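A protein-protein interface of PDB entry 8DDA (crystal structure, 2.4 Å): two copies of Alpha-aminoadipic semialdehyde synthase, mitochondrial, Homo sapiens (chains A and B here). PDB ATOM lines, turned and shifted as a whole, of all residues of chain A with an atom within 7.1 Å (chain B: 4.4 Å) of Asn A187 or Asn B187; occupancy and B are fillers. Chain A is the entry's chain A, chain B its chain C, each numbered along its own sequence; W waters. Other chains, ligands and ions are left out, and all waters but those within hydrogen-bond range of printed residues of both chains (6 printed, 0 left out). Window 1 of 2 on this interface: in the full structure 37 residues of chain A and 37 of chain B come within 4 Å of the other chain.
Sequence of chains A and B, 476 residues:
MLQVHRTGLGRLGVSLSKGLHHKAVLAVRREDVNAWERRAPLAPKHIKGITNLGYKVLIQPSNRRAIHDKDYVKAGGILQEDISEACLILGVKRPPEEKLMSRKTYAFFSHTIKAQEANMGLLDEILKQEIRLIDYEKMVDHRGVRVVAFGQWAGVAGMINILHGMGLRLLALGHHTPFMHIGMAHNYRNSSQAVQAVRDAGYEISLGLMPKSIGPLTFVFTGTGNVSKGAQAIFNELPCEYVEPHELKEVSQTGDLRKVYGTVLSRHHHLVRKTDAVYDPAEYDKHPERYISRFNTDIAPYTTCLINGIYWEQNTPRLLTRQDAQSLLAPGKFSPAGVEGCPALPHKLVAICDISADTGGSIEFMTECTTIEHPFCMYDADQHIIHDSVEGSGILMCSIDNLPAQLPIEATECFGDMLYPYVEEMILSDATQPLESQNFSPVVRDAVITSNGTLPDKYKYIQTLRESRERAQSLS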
ATOM      1  N   ARG A  38      -6.628 -15.792  -2.535  1.00  0.00           N
ATOM      2  CA  ARG A  38      -5.829 -15.088  -1.502  1.00  0.00           C
ATOM      3  C   ARG A  38      -4.354 -15.034  -1.922  1.00  0.00           C
ATOM      4  O   ARG A  38      -3.565 -14.466  -1.133  1.00  0.00           O
ATOM      5  CB  ARG A  38      -5.988 -15.772  -0.139  1.00  0.00           C
ATOM      6  CG  ARG A  38      -7.376 -15.641   0.478  1.00  0.00           C
ATOM      7  CD  ARG A  38      -7.448 -16.090   1.931  1.00  0.00           C
ATOM      8  NE  ARG A  38      -7.472 -17.544   2.003  1.00  0.00           N
ATOM      9  CZ  ARG A  38      -6.956 -18.312   2.973  1.00  0.00           C
ATOM     10  NH1 ARG A  38      -6.372 -17.811   4.045  1.00  0.00           N
ATOM     11  NH2 ARG A  38      -7.056 -19.614   2.853  1.00  0.00           N
ATOM     12  N   HIS A 164      -9.035 -35.338   6.238  1.00  0.00           N
ATOM     13  CA  HIS A 164     -10.250 -34.734   6.853  1.00  0.00           C
ATOM     14  C   HIS A 164     -11.516 -35.455   6.343  1.00  0.00           C
ATOM     15  O   HIS A 164     -12.354 -35.898   7.175  1.00  0.00           O
ATOM     16  CB  HIS A 164     -10.274 -33.230   6.569  1.00  0.00           C
ATOM     17  CG  HIS A 164     -11.541 -32.538   6.956  1.00  0.00           C
ATOM     18  ND1 HIS A 164     -11.854 -32.235   8.263  1.00  0.00           N
ATOM     19  CD2 HIS A 164     -12.550 -32.047   6.209  1.00  0.00           C
ATOM     20  CE1 HIS A 164     -13.000 -31.589   8.303  1.00  0.00           C
ATOM     21  NE2 HIS A 164     -13.447 -31.467   7.056  1.00  0.00           N
ATOM     22  N   LEU A 168     -14.744 -37.684   8.462  1.00  0.00           N
ATOM     23  CA  LEU A 168     -16.208 -37.452   8.354  1.00  0.00           C
ATOM     24  C   LEU A 168     -16.898 -38.685   7.758  1.00  0.00           C
ATOM     25  O   LEU A 168     -17.916 -39.134   8.330  1.00  0.00           O
ATOM     26  CB  LEU A 168     -16.440 -36.219   7.478  1.00  0.00           C
ATOM     27  CG  LEU A 168     -15.915 -34.903   8.037  1.00  0.00           C
ATOM     28  CD1 LEU A 168     -16.325 -33.724   7.174  1.00  0.00           C
ATOM     29  CD2 LEU A 168     -16.438 -34.681   9.442  1.00  0.00           C
ATOM     30  N   PRO A 178      -9.001 -41.101  14.687  1.00  0.00           N
ATOM     31  CA  PRO A 178      -8.132 -39.926  14.779  1.00  0.00           C
ATOM     32  C   PRO A 178      -8.148 -38.964  13.571  1.00  0.00           C
ATOM     33  O   PRO A 178      -7.741 -37.815  13.729  1.00  0.00           O
ATOM     34  CB  PRO A 178      -6.741 -40.557  14.954  1.00  0.00           C
ATOM     35  CG  PRO A 178      -7.029 -41.910  15.574  1.00  0.00           C
ATOM     36  CD  PRO A 178      -8.266 -42.368  14.835  1.00  0.00           C
ATOM     37  N   PHE A 179      -8.643 -39.399  12.410  1.00  0.00           N
ATOM     38  CA  PHE A 179      -8.808 -38.515  11.217  1.00  0.00           C
ATOM     39  C   PHE A 179      -9.840 -37.408  11.515  1.00  0.00           C
ATOM     40  O   PHE A 179      -9.826 -36.358  10.832  1.00  0.00           O
ATOM     41  CB  PHE A 179      -9.121 -39.344   9.969  1.00  0.00           C
ATOM     42  CG  PHE A 179      -8.014 -40.289   9.570  1.00  0.00           C
ATOM     43  CD1 PHE A 179      -6.710 -39.833   9.416  1.00  0.00           C
ATOM     44  CD2 PHE A 179      -8.272 -41.634   9.340  1.00  0.00           C
ATOM     45  CE1 PHE A 179      -5.690 -40.702   9.046  1.00  0.00           C
ATOM     46  CE2 PHE A 179      -7.250 -42.506   8.990  1.00  0.00           C
ATOM     47  CZ  PHE A 179      -5.966 -42.034   8.825  1.00  0.00           C
ATOM     48  N   MET A 180     -10.679 -37.580  12.537  1.00  0.00           N
ATOM     49  CA  MET A 180     -11.578 -36.480  13.010  1.00  0.00           C
ATOM     50  C   MET A 180     -10.757 -35.256  13.444  1.00  0.00           C
ATOM     51  O   MET A 180     -11.355 -34.153  13.495  1.00  0.00           O
ATOM     52  CB  MET A 180     -12.471 -36.908  14.182  1.00  0.00           C
ATOM     53  CG  MET A 180     -13.598 -37.837  13.789  1.00  0.00           C
ATOM     54  SD  MET A 180     -14.748 -37.138  12.563  1.00  0.00           S
ATOM     55  CE  MET A 180     -15.376 -35.726  13.483  1.00  0.00           C
ATOM     56  N   HIS A 181      -9.461 -35.412  13.762  1.00  0.00           N
ATOM     57  CA  HIS A 181      -8.639 -34.337  14.405  1.00  0.00           C
ATOM     58  C   HIS A 181      -7.766 -33.613  13.363  1.00  0.00           C
ATOM     59  O   HIS A 181      -6.767 -32.948  13.768  1.00  0.00           O
ATOM     60  CB  HIS A 181      -7.848 -34.934  15.571  1.00  0.00           C
ATOM     61  CG  HIS A 181      -8.715 -35.622  16.575  1.00  0.00           C
ATOM     62  ND1 HIS A 181      -8.286 -36.731  17.300  1.00  0.00           N
ATOM     63  CD2 HIS A 181      -9.973 -35.372  16.994  1.00  0.00           C
ATOM     64  CE1 HIS A 181      -9.253 -37.146  18.095  1.00  0.00           C
ATOM     65  NE2 HIS A 181     -10.293 -36.336  17.924  1.00  0.00           N
ATOM     66  N   ILE A 182      -8.093 -33.770  12.072  1.00  0.00           N
ATOM     67  CA  ILE A 182      -7.453 -33.057  10.924  1.00  0.00           C
ATOM     68  C   ILE A 182      -8.521 -32.205  10.237  1.00  0.00           C
ATOM     69  O   ILE A 182      -9.568 -32.778   9.850  1.00  0.00           O
ATOM     70  CB  ILE A 182      -6.811 -34.063   9.952  1.00  0.00           C
ATOM     71  CG1 ILE A 182      -5.839 -34.987  10.690  1.00  0.00           C
ATOM     72  CG2 ILE A 182      -6.151 -33.335   8.792  1.00  0.00           C
ATOM     73  CD1 ILE A 182      -5.156 -36.029   9.837  1.00  0.00           C
ATOM     74  N   GLY A 183      -8.305 -30.893  10.121  1.00  0.00           N
ATOM     75  CA  GLY A 183      -9.281 -29.995   9.462  1.00  0.00           C
ATOM     76  C   GLY A 183      -9.003 -29.896   7.967  1.00  0.00           C
ATOM     77  O   GLY A 183      -8.168 -30.678   7.466  1.00  0.00           O
ATOM     78  N   MET A 184      -9.667 -28.963   7.288  1.00  0.00           N
ATOM     79  CA  MET A 184      -9.410 -28.611   5.866  1.00  0.00           C
ATOM     80  C   MET A 184      -8.103 -27.810   5.816  1.00  0.00           C
ATOM     81  O   MET A 184      -7.808 -27.070   6.798  1.00  0.00           O
ATOM     82  CB  MET A 184     -10.550 -27.762   5.291  1.00  0.00           C
ATOM     83  CG  MET A 184     -11.896 -28.483   5.145  1.00  0.00           C
ATOM     84  SD  MET A 184     -11.884 -29.706   3.789  1.00  0.00           S
ATOM     85  CE  MET A 184     -11.853 -28.633   2.355  1.00  0.00           C
ATOM     86  N   ALA A 185      -7.375 -27.906   4.700  1.00  0.00           N
ATOM     87  CA  ALA A 185      -6.060 -27.263   4.493  1.00  0.00           C
ATOM     88  C   ALA A 185      -6.109 -25.770   4.848  1.00  0.00           C
ATOM     89  O   ALA A 185      -5.121 -25.266   5.437  1.00  0.00           O
ATOM     90  CB  ALA A 185      -5.580 -27.510   3.091  1.00  0.00           C
ATOM     91  N   HIS A 186      -7.213 -25.083   4.544  1.00  0.00           N
ATOM     92  CA  HIS A 186      -7.350 -23.613   4.764  1.00  0.00           C
ATOM     93  C   HIS A 186      -7.636 -23.258   6.241  1.00  0.00           C
ATOM     94  O   HIS A 186      -7.631 -22.076   6.534  1.00  0.00           O
ATOM     95  CB  HIS A 186      -8.395 -23.040   3.811  1.00  0.00           C
ATOM     96  CG  HIS A 186      -9.768 -23.602   3.975  1.00  0.00           C
ATOM     97  ND1 HIS A 186     -10.231 -24.636   3.181  1.00  0.00           N
ATOM     98  CD2 HIS A 186     -10.800 -23.230   4.777  1.00  0.00           C
ATOM     99  CE1 HIS A 186     -11.487 -24.895   3.510  1.00  0.00           C
ATOM    100  NE2 HIS A 186     -11.856 -24.037   4.501  1.00  0.00           N
ATOM    101  N   ASN A 187      -7.864 -24.231   7.131  1.00  0.00           N
ATOM    102  CA  ASN A 187      -8.071 -24.012   8.588  1.00  0.00           C
ATOM    103  C   ASN A 187      -6.696 -23.896   9.296  1.00  0.00           C
ATOM    104  O   ASN A 187      -6.678 -23.644  10.550  1.00  0.00           O
ATOM    105  CB  ASN A 187      -8.918 -25.131   9.232  1.00  0.00           C
ATOM    106  CG  ASN A 187     -10.332 -25.273   8.689  1.00  0.00           C
ATOM    107  OD1 ASN A 187     -10.876 -26.398   8.604  1.00  0.00           O
ATOM    108  ND2 ASN A 187     -10.955 -24.142   8.347  1.00  0.00           N
ATOM    109  N   TYR A 188      -5.569 -24.052   8.569  1.00  0.00           N
ATOM    110  CA  TYR A 188      -4.195 -24.031   9.145  1.00  0.00           C
ATOM    111  C   TYR A 188      -3.440 -22.787   8.652  1.00  0.00           C
ATOM    112  O   TYR A 188      -3.658 -22.407   7.486  1.00  0.00           O
ATOM    113  CB  TYR A 188      -3.464 -25.341   8.830  1.00  0.00           C
ATOM    114  CG  TYR A 188      -4.081 -26.568   9.462  1.00  0.00           C
ATOM    115  CD1 TYR A 188      -4.100 -26.738  10.842  1.00  0.00           C
ATOM    116  CD2 TYR A 188      -4.651 -27.575   8.696  1.00  0.00           C
ATOM    117  CE1 TYR A 188      -4.715 -27.834  11.436  1.00  0.00           C
ATOM    118  CE2 TYR A 188      -5.216 -28.705   9.271  1.00  0.00           C
ATOM    119  CZ  TYR A 188      -5.255 -28.831  10.647  1.00  0.00           C
ATOM    120  OH  TYR A 188      -5.836 -29.917  11.242  1.00  0.00           O
ATOM    121  N   ARG A 189      -2.572 -22.200   9.493  1.00  0.00           N
ATOM    122  CA  ARG A 189      -1.786 -20.978   9.169  1.00  0.00           C
ATOM    123  C   ARG A 189      -0.888 -21.216   7.944  1.00  0.00           C
ATOM    124  O   ARG A 189      -0.711 -20.275   7.148  1.00  0.00           O
ATOM    125  CB  ARG A 189      -0.955 -20.533  10.386  1.00  0.00           C
ATOM    126  CG  ARG A 189      -0.117 -19.282  10.136  1.00  0.00           C
ATOM    127  CD  ARG A 189       0.643 -18.717  11.339  1.00  0.00           C
ATOM    128  NE  ARG A 189       1.755 -19.549  11.793  1.00  0.00           N
ATOM    129  CZ  ARG A 189       1.662 -20.549  12.675  1.00  0.00           C
ATOM    130  NH1 ARG A 189       0.512 -20.859  13.246  1.00  0.00           N
ATOM    131  NH2 ARG A 189       2.717 -21.261  13.000  1.00  0.00           N
ATOM    132  N   ASN A 190      -0.294 -22.411   7.836  1.00  0.00           N
ATOM    133  CA  ASN A 190       0.673 -22.816   6.777  1.00  0.00           C
ATOM    134  C   ASN A 190       0.873 -24.342   6.855  1.00  0.00           C
ATOM    135  O   ASN A 190       0.316 -24.958   7.787  1.00  0.00           O
ATOM    136  CB  ASN A 190       2.004 -22.054   6.922  1.00  0.00           C
ATOM    137  CG  ASN A 190       2.650 -22.250   8.281  1.00  0.00           C
ATOM    138  OD1 ASN A 190       2.544 -23.319   8.873  1.00  0.00           O
ATOM    139  ND2 ASN A 190       3.291 -21.221   8.820  1.00  0.00           N
ATOM    140  N   GLN A 193       1.895 -25.853  10.441  1.00  0.00           N
ATOM    141  CA  GLN A 193       0.823 -26.033  11.456  1.00  0.00           C
ATOM    142  C   GLN A 193       0.032 -27.278  11.045  1.00  0.00           C
ATOM    143  O   GLN A 193      -0.263 -28.102  11.923  1.00  0.00           O
ATOM    144  CB  GLN A 193      -0.060 -24.782  11.611  1.00  0.00           C
ATOM    145  CG  GLN A 193      -0.844 -24.775  12.918  1.00  0.00           C
ATOM    146  CD  GLN A 193      -1.896 -23.695  13.019  1.00  0.00           C
ATOM    147  OE1 GLN A 193      -2.714 -23.478  12.103  1.00  0.00           O
ATOM    148  NE2 GLN A 193      -1.895 -23.031  14.161  1.00  0.00           N
ATOM    149  N   ALA A 197      -0.611 -31.148  13.169  1.00  0.00           N
ATOM    150  CA  ALA A 197      -1.938 -31.789  13.338  1.00  0.00           C
ATOM    151  C   ALA A 197      -1.944 -33.206  12.747  1.00  0.00           C
ATOM    152  O   ALA A 197      -2.555 -34.129  13.393  1.00  0.00           O
ATOM    153  CB  ALA A 197      -2.994 -30.924  12.735  1.00  0.00           C
ATOM    154  N   GLN A 406      -5.698 -22.885  -1.024  1.00  0.00           N
ATOM    155  CA  GLN A 406      -5.899 -23.264   0.398  1.00  0.00           C
ATOM    156  C   GLN A 406      -4.597 -23.087   1.212  1.00  0.00           C
ATOM    157  O   GLN A 406      -4.690 -23.084   2.468  1.00  0.00           O
ATOM    158  CB  GLN A 406      -6.364 -24.707   0.534  1.00  0.00           C
ATOM    159  CG  GLN A 406      -7.677 -24.990  -0.173  1.00  0.00           C
ATOM    160  CD  GLN A 406      -8.113 -26.405   0.095  1.00  0.00           C
ATOM    161  OE1 GLN A 406      -7.785 -27.319  -0.666  1.00  0.00           O
ATOM    162  NE2 GLN A 406      -8.779 -26.607   1.219  1.00  0.00           N
ATOM    163  N   HIS B 164     -14.189 -19.462  14.064  1.00  0.00           N
ATOM    164  CA  HIS B 164     -14.145 -20.070  12.704  1.00  0.00           C
ATOM    165  C   HIS B 164     -15.154 -19.367  11.774  1.00  0.00           C
ATOM    166  O   HIS B 164     -14.766 -18.926  10.656  1.00  0.00           O
ATOM    167  CB  HIS B 164     -14.391 -21.578  12.805  1.00  0.00           C
ATOM    168  CG  HIS B 164     -14.573 -22.274  11.500  1.00  0.00           C
ATOM    169  ND1 HIS B 164     -13.515 -22.566  10.671  1.00  0.00           N
ATOM    170  CD2 HIS B 164     -15.682 -22.773  10.897  1.00  0.00           C
ATOM    171  CE1 HIS B 164     -13.951 -23.231   9.616  1.00  0.00           C
ATOM    172  NE2 HIS B 164     -15.284 -23.368   9.729  1.00  0.00           N
ATOM    173  N   MET B 180      -9.199 -17.159   9.937  1.00  0.00           N
ATOM    174  CA  MET B 180      -9.135 -18.251   8.932  1.00  0.00           C
ATOM    175  C   MET B 180      -8.384 -19.467   9.480  1.00  0.00           C
ATOM    176  O   MET B 180      -8.576 -20.553   8.909  1.00  0.00           O
ATOM    177  CB  MET B 180      -8.442 -17.800   7.633  1.00  0.00           C
ATOM    178  CG  MET B 180      -9.317 -16.877   6.766  1.00  0.00           C
ATOM    179  SD  MET B 180     -10.882 -17.663   6.225  1.00  0.00           S
ATOM    180  CE  MET B 180     -10.251 -19.077   5.319  1.00  0.00           C
ATOM    181  N   HIS B 181      -7.543 -19.308  10.516  1.00  0.00           N
ATOM    182  CA  HIS B 181      -6.608 -20.372  10.999  1.00  0.00           C
ATOM    183  C   HIS B 181      -7.174 -21.079  12.245  1.00  0.00           C
ATOM    184  O   HIS B 181      -6.386 -21.741  12.962  1.00  0.00           O
ATOM    185  CB  HIS B 181      -5.210 -19.768  11.205  1.00  0.00           C
ATOM    186  CG  HIS B 181      -4.676 -19.087   9.993  1.00  0.00           C
ATOM    187  ND1 HIS B 181      -3.839 -17.979  10.074  1.00  0.00           N
ATOM    188  CD2 HIS B 181      -4.826 -19.367   8.673  1.00  0.00           C
ATOM    189  CE1 HIS B 181      -3.519 -17.579   8.852  1.00  0.00           C
ATOM    190  NE2 HIS B 181      -4.130 -18.416   7.966  1.00  0.00           N
ATOM    191  N   ILE B 182      -8.476 -20.951  12.492  1.00  0.00           N
ATOM    192  CA  ILE B 182      -9.232 -21.677  13.562  1.00  0.00           C
ATOM    193  C   ILE B 182     -10.311 -22.535  12.877  1.00  0.00           C
ATOM    194  O   ILE B 182     -11.110 -21.972  12.084  1.00  0.00           O
ATOM    195  CB  ILE B 182      -9.852 -20.683  14.563  1.00  0.00           C
ATOM    196  CG1 ILE B 182      -8.781 -19.774  15.156  1.00  0.00           C
ATOM    197  CG2 ILE B 182     -10.626 -21.417  15.646  1.00  0.00           C
ATOM    198  CD1 ILE B 182      -9.288 -18.746  16.152  1.00  0.00           C
ATOM    199  N   GLY B 183     -10.332 -23.841  13.150  1.00  0.00           N
ATOM    200  CA  GLY B 183     -11.328 -24.748  12.528  1.00  0.00           C
ATOM    201  C   GLY B 183     -12.555 -24.861  13.414  1.00  0.00           C
ATOM    202  O   GLY B 183     -12.664 -24.075  14.382  1.00  0.00           O
ATOM    203  N   MET B 184     -13.434 -25.814  13.108  1.00  0.00           N
ATOM    204  CA  MET B 184     -14.607 -26.184  13.939  1.00  0.00           C
ATOM    205  C   MET B 184     -14.094 -26.964  15.150  1.00  0.00           C
ATOM    206  O   MET B 184     -13.073 -27.688  15.008  1.00  0.00           O
ATOM    207  CB  MET B 184     -15.593 -27.054  13.135  1.00  0.00           C
ATOM    208  CG  MET B 184     -16.316 -26.324  12.000  1.00  0.00           C
ATOM    209  SD  MET B 184     -17.548 -25.101  12.577  1.00  0.00           S
ATOM    210  CE  MET B 184     -18.818 -26.203  13.210  1.00  0.00           C
ATOM    211  N   ALA B 185     -14.812 -26.893  16.265  1.00  0.00           N
ATOM    212  CA  ALA B 185     -14.419 -27.510  17.557  1.00  0.00           C
ATOM    213  C   ALA B 185     -14.098 -28.995  17.384  1.00  0.00           C
ATOM    214  O   ALA B 185     -13.143 -29.483  18.034  1.00  0.00           O
ATOM    215  CB  ALA B 185     -15.485 -27.273  18.602  1.00  0.00           C
ATOM    216  N   HIS B 186     -14.832 -29.701  16.524  1.00  0.00           N
ATOM    217  CA  HIS B 186     -14.666 -31.172  16.329  1.00  0.00           C
ATOM    218  C   HIS B 186     -13.451 -31.516  15.450  1.00  0.00           C
ATOM    219  O   HIS B 186     -13.152 -32.707  15.367  1.00  0.00           O
ATOM    220  CB  HIS B 186     -15.963 -31.788  15.790  1.00  0.00           C
ATOM    221  CG  HIS B 186     -16.410 -31.247  14.476  1.00  0.00           C
ATOM    222  ND1 HIS B 186     -17.305 -30.191  14.367  1.00  0.00           N
ATOM    223  CD2 HIS B 186     -16.130 -31.646  13.215  1.00  0.00           C
ATOM    224  CE1 HIS B 186     -17.547 -29.946  13.093  1.00  0.00           C
ATOM    225  NE2 HIS B 186     -16.834 -30.836  12.366  1.00  0.00           N
ATOM    226  N   ASN B 187     -12.767 -30.532  14.851  1.00  0.00           N
ATOM    227  CA  ASN B 187     -11.524 -30.738  14.057  1.00  0.00           C
ATOM    228  C   ASN B 187     -10.299 -30.857  15.001  1.00  0.00           C
ATOM    229  O   ASN B 187      -9.179 -31.091  14.492  1.00  0.00           O
ATOM    230  CB  ASN B 187     -11.313 -29.628  13.003  1.00  0.00           C
ATOM    231  CG  ASN B 187     -12.412 -29.503  11.954  1.00  0.00           C
ATOM    232  OD1 ASN B 187     -12.716 -28.393  11.468  1.00  0.00           O
ATOM    233  ND2 ASN B 187     -12.988 -30.628  11.556  1.00  0.00           N
ATOM    234  N   TYR B 188     -10.478 -30.702  16.324  1.00  0.00           N
ATOM    235  CA  TYR B 188      -9.365 -30.690  17.330  1.00  0.00           C
ATOM    236  C   TYR B 188      -9.491 -31.897  18.266  1.00  0.00           C
ATOM    237  O   TYR B 188     -10.635 -32.276  18.569  1.00  0.00           O
ATOM    238  CB  TYR B 188      -9.359 -29.363  18.098  1.00  0.00           C
ATOM    239  CG  TYR B 188      -9.062 -28.145  17.257  1.00  0.00           C
ATOM    240  CD1 TYR B 188      -7.829 -27.971  16.659  1.00  0.00           C
ATOM    241  CD2 TYR B 188     -10.016 -27.169  17.042  1.00  0.00           C
ATOM    242  CE1 TYR B 188      -7.549 -26.859  15.873  1.00  0.00           C
ATOM    243  CE2 TYR B 188      -9.753 -26.054  16.264  1.00  0.00           C
ATOM    244  CZ  TYR B 188      -8.513 -25.891  15.679  1.00  0.00           C
ATOM    245  OH  TYR B 188      -8.262 -24.802  14.896  1.00  0.00           O
ATOM    246  N   GLN B 193      -5.676 -28.732  22.248  1.00  0.00           N
ATOM    247  CA  GLN B 193      -5.204 -28.562  20.850  1.00  0.00           C
ATOM    248  C   GLN B 193      -5.919 -27.339  20.304  1.00  0.00           C
ATOM    249  O   GLN B 193      -5.272 -26.523  19.656  1.00  0.00           O
ATOM    250  CB  GLN B 193      -5.424 -29.823  19.991  1.00  0.00           C
ATOM    251  CG  GLN B 193      -4.578 -29.838  18.719  1.00  0.00           C
ATOM    252  CD  GLN B 193      -4.898 -30.979  17.778  1.00  0.00           C
ATOM    253  OE1 GLN B 193      -6.060 -31.243  17.462  1.00  0.00           O
ATOM    254  NE2 GLN B 193      -3.883 -31.669  17.306  1.00  0.00           N
HETATM  255  O   HOH W   1      -6.756 -29.736  13.861  1.00  0.00           O
HETATM  256  O   HOH W   2      -3.669 -18.376   5.378  1.00  0.00           O
HETATM  257  O   HOH W   3      -4.418 -33.780  15.279  1.00  0.00           O
HETATM  258  O   HOH W   4      -3.970 -20.871  14.282  1.00  0.00           O
HETATM  259  O   HOH W   5      -6.141 -25.017  13.192  1.00  0.00           O
HETATM  260  O   HOH W   6     -13.181 -33.145  11.922  1.00  0.00           O
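The backbone carbonyl oxygen of Met A180 sits close to the backbone carbonyl oxygen of His B186. O of His A181 lies close to O of Asn B187, 3.1 Å away. The backbone carbonyl oxygen (O) of Met B180 lies close to the backbone carbonyl oxygen (O) of His A186, 3.0 Å away. The backbone carbonyl oxygen (O) of His B181 lies close to the backbone carbonyl oxygen (O) of Asn A187.
A ring nitrogen (ND1) of His A164 lies within hydrogen-bond range of the backbone carbonyl oxygen (O) of Ile A182. The backbone NH (N) of Gly A183 sits at hydrogen-bond distance from the side-chain hydroxyl (OH) of Tyr A188 (2.9 Å). The backbone NH (N) of Met A184 sits at hydrogen-bond distance from the side-chain amide oxygen (OD1) of Asn A187, 3.1 Å away. A ring nitrogen (ND1) of His A186 lies within hydrogen-bond range of the side-chain amide nitrogen of Gln A406 (3.1 Å). A ring nitrogen (ND1) of His B164 sits at hydrogen-bond distance from the backbone carbonyl oxygen (O) of Ile B182 (2.9 Å). The side-chain hydroxyl (OH) of Tyr B188 is in hydrogen-bond range of the backbone NH (N) of Gly B183, 2.9 Å away.
His A164 touches Asn B187. Asn B187 touches Met A180. His A181 touches Tyr B188. Asn B187 touches Ile A182 (O to N, 3.8 Å). CE1 of His B164 touches ND2 of Asn A187 (3.4 Å). Met B180 touches Asn A187 (O to CA, 3.5 Å). Asn A187 touches Ile B182 (O to N, 3.8 Å). Asn A187 touches Asn B187. His B181 touches Tyr A188 (CD2 to O, 3.5 Å). CD2 of His B181 touches CA of Arg A189 (3.5 Å).
Printed residues of chain B within 4 Å of Asn A187: His B164 (3.4 Å), Met B180 (3.5 Å), His B181 (3.1 Å), Ile B182 (3.8 Å) and Asn B187 (3.9 Å). Asn B187 touches five residues of chain A. Of the printed residues of chain B, Ile A182 touches Asn B187 (3.8 Å). Of the printed residues of chain B, Met A180 touches His B186 and Asn B187. Gln A406 touches none of the printed residues of chain B. Met B184 touches none of the printed residues of chain A. The nearest printed residue of chain B that does not touch Asn A187 is Gly B183 (4.001 Å). The nearest residue of chain A that does not touch Asn B187 is Gly A183 (4.03 Å). The nearest printed residue of chain A that does not touch His B181 is Gln A193 (4.2 Å).
Printed residues of chain A that touch a printed residue of chain B: His A164, Met A180, His A181, Ile A182, His A186, Asn A187, Tyr A188 and Arg A189. Hydrophobic or aromatic side chains of chain A within 4 Å of the printed part of chain B: His A164 and His A181. Among the printed residues, 14 pairs touch across the chains.
Met A180 touches His B186, and with the chains exchanged His A186 touches Met B180. Met A180 touches Asn B187, and with the chains exchanged Asn A187 touches Met B180. Ile A182 touches Asn B187, and with the chains exchanged Asn A187 touches Ile B182. Asn A187 touches its own counterpart, Asn B187.
Water W6 lies within hydrogen-bond range of the side-chain amide nitrogen of Asn B187 (2.6 Å), the backbone carbonyl oxygen of Met A180 (2.6 Å) and the backbone carbonyl oxygen of His B186 (3.5 Å). Water W2 bridges a ring nitrogen (NE2) of His B181 (2.6 Å) and the guanidinium group (NH1) of Arg A38 (3.1 Å). Water W3 lies within hydrogen-bond range of the backbone carbonyl oxygen (O) of Ala A197 (2.7 Å), the backbone carbonyl oxygen (O) of His A181 (2.9 Å) and the side-chain amide nitrogen (NE2) of Gln B193 (3.0 Å). Water W5 lies within hydrogen-bond range of the side-chain hydroxyl (OH) of Tyr B188, the backbone carbonyl oxygen (O) of Asn A187 and the backbone carbonyl oxygen (O) of His B181. Water W1 lies within hydrogen-bond range of the side-chain hydroxyl of Tyr A188 (2.8 Å), the backbone carbonyl oxygen of Asn B187 (2.8 Å) and the backbone carbonyl oxygen of His A181 (3.2 Å). Water W4 lies within hydrogen-bond range of the backbone carbonyl oxygen (O) of His B181 (2.9 Å) and the side-chain amide nitrogen (NE2) of Gln A193 (3.0 Å).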
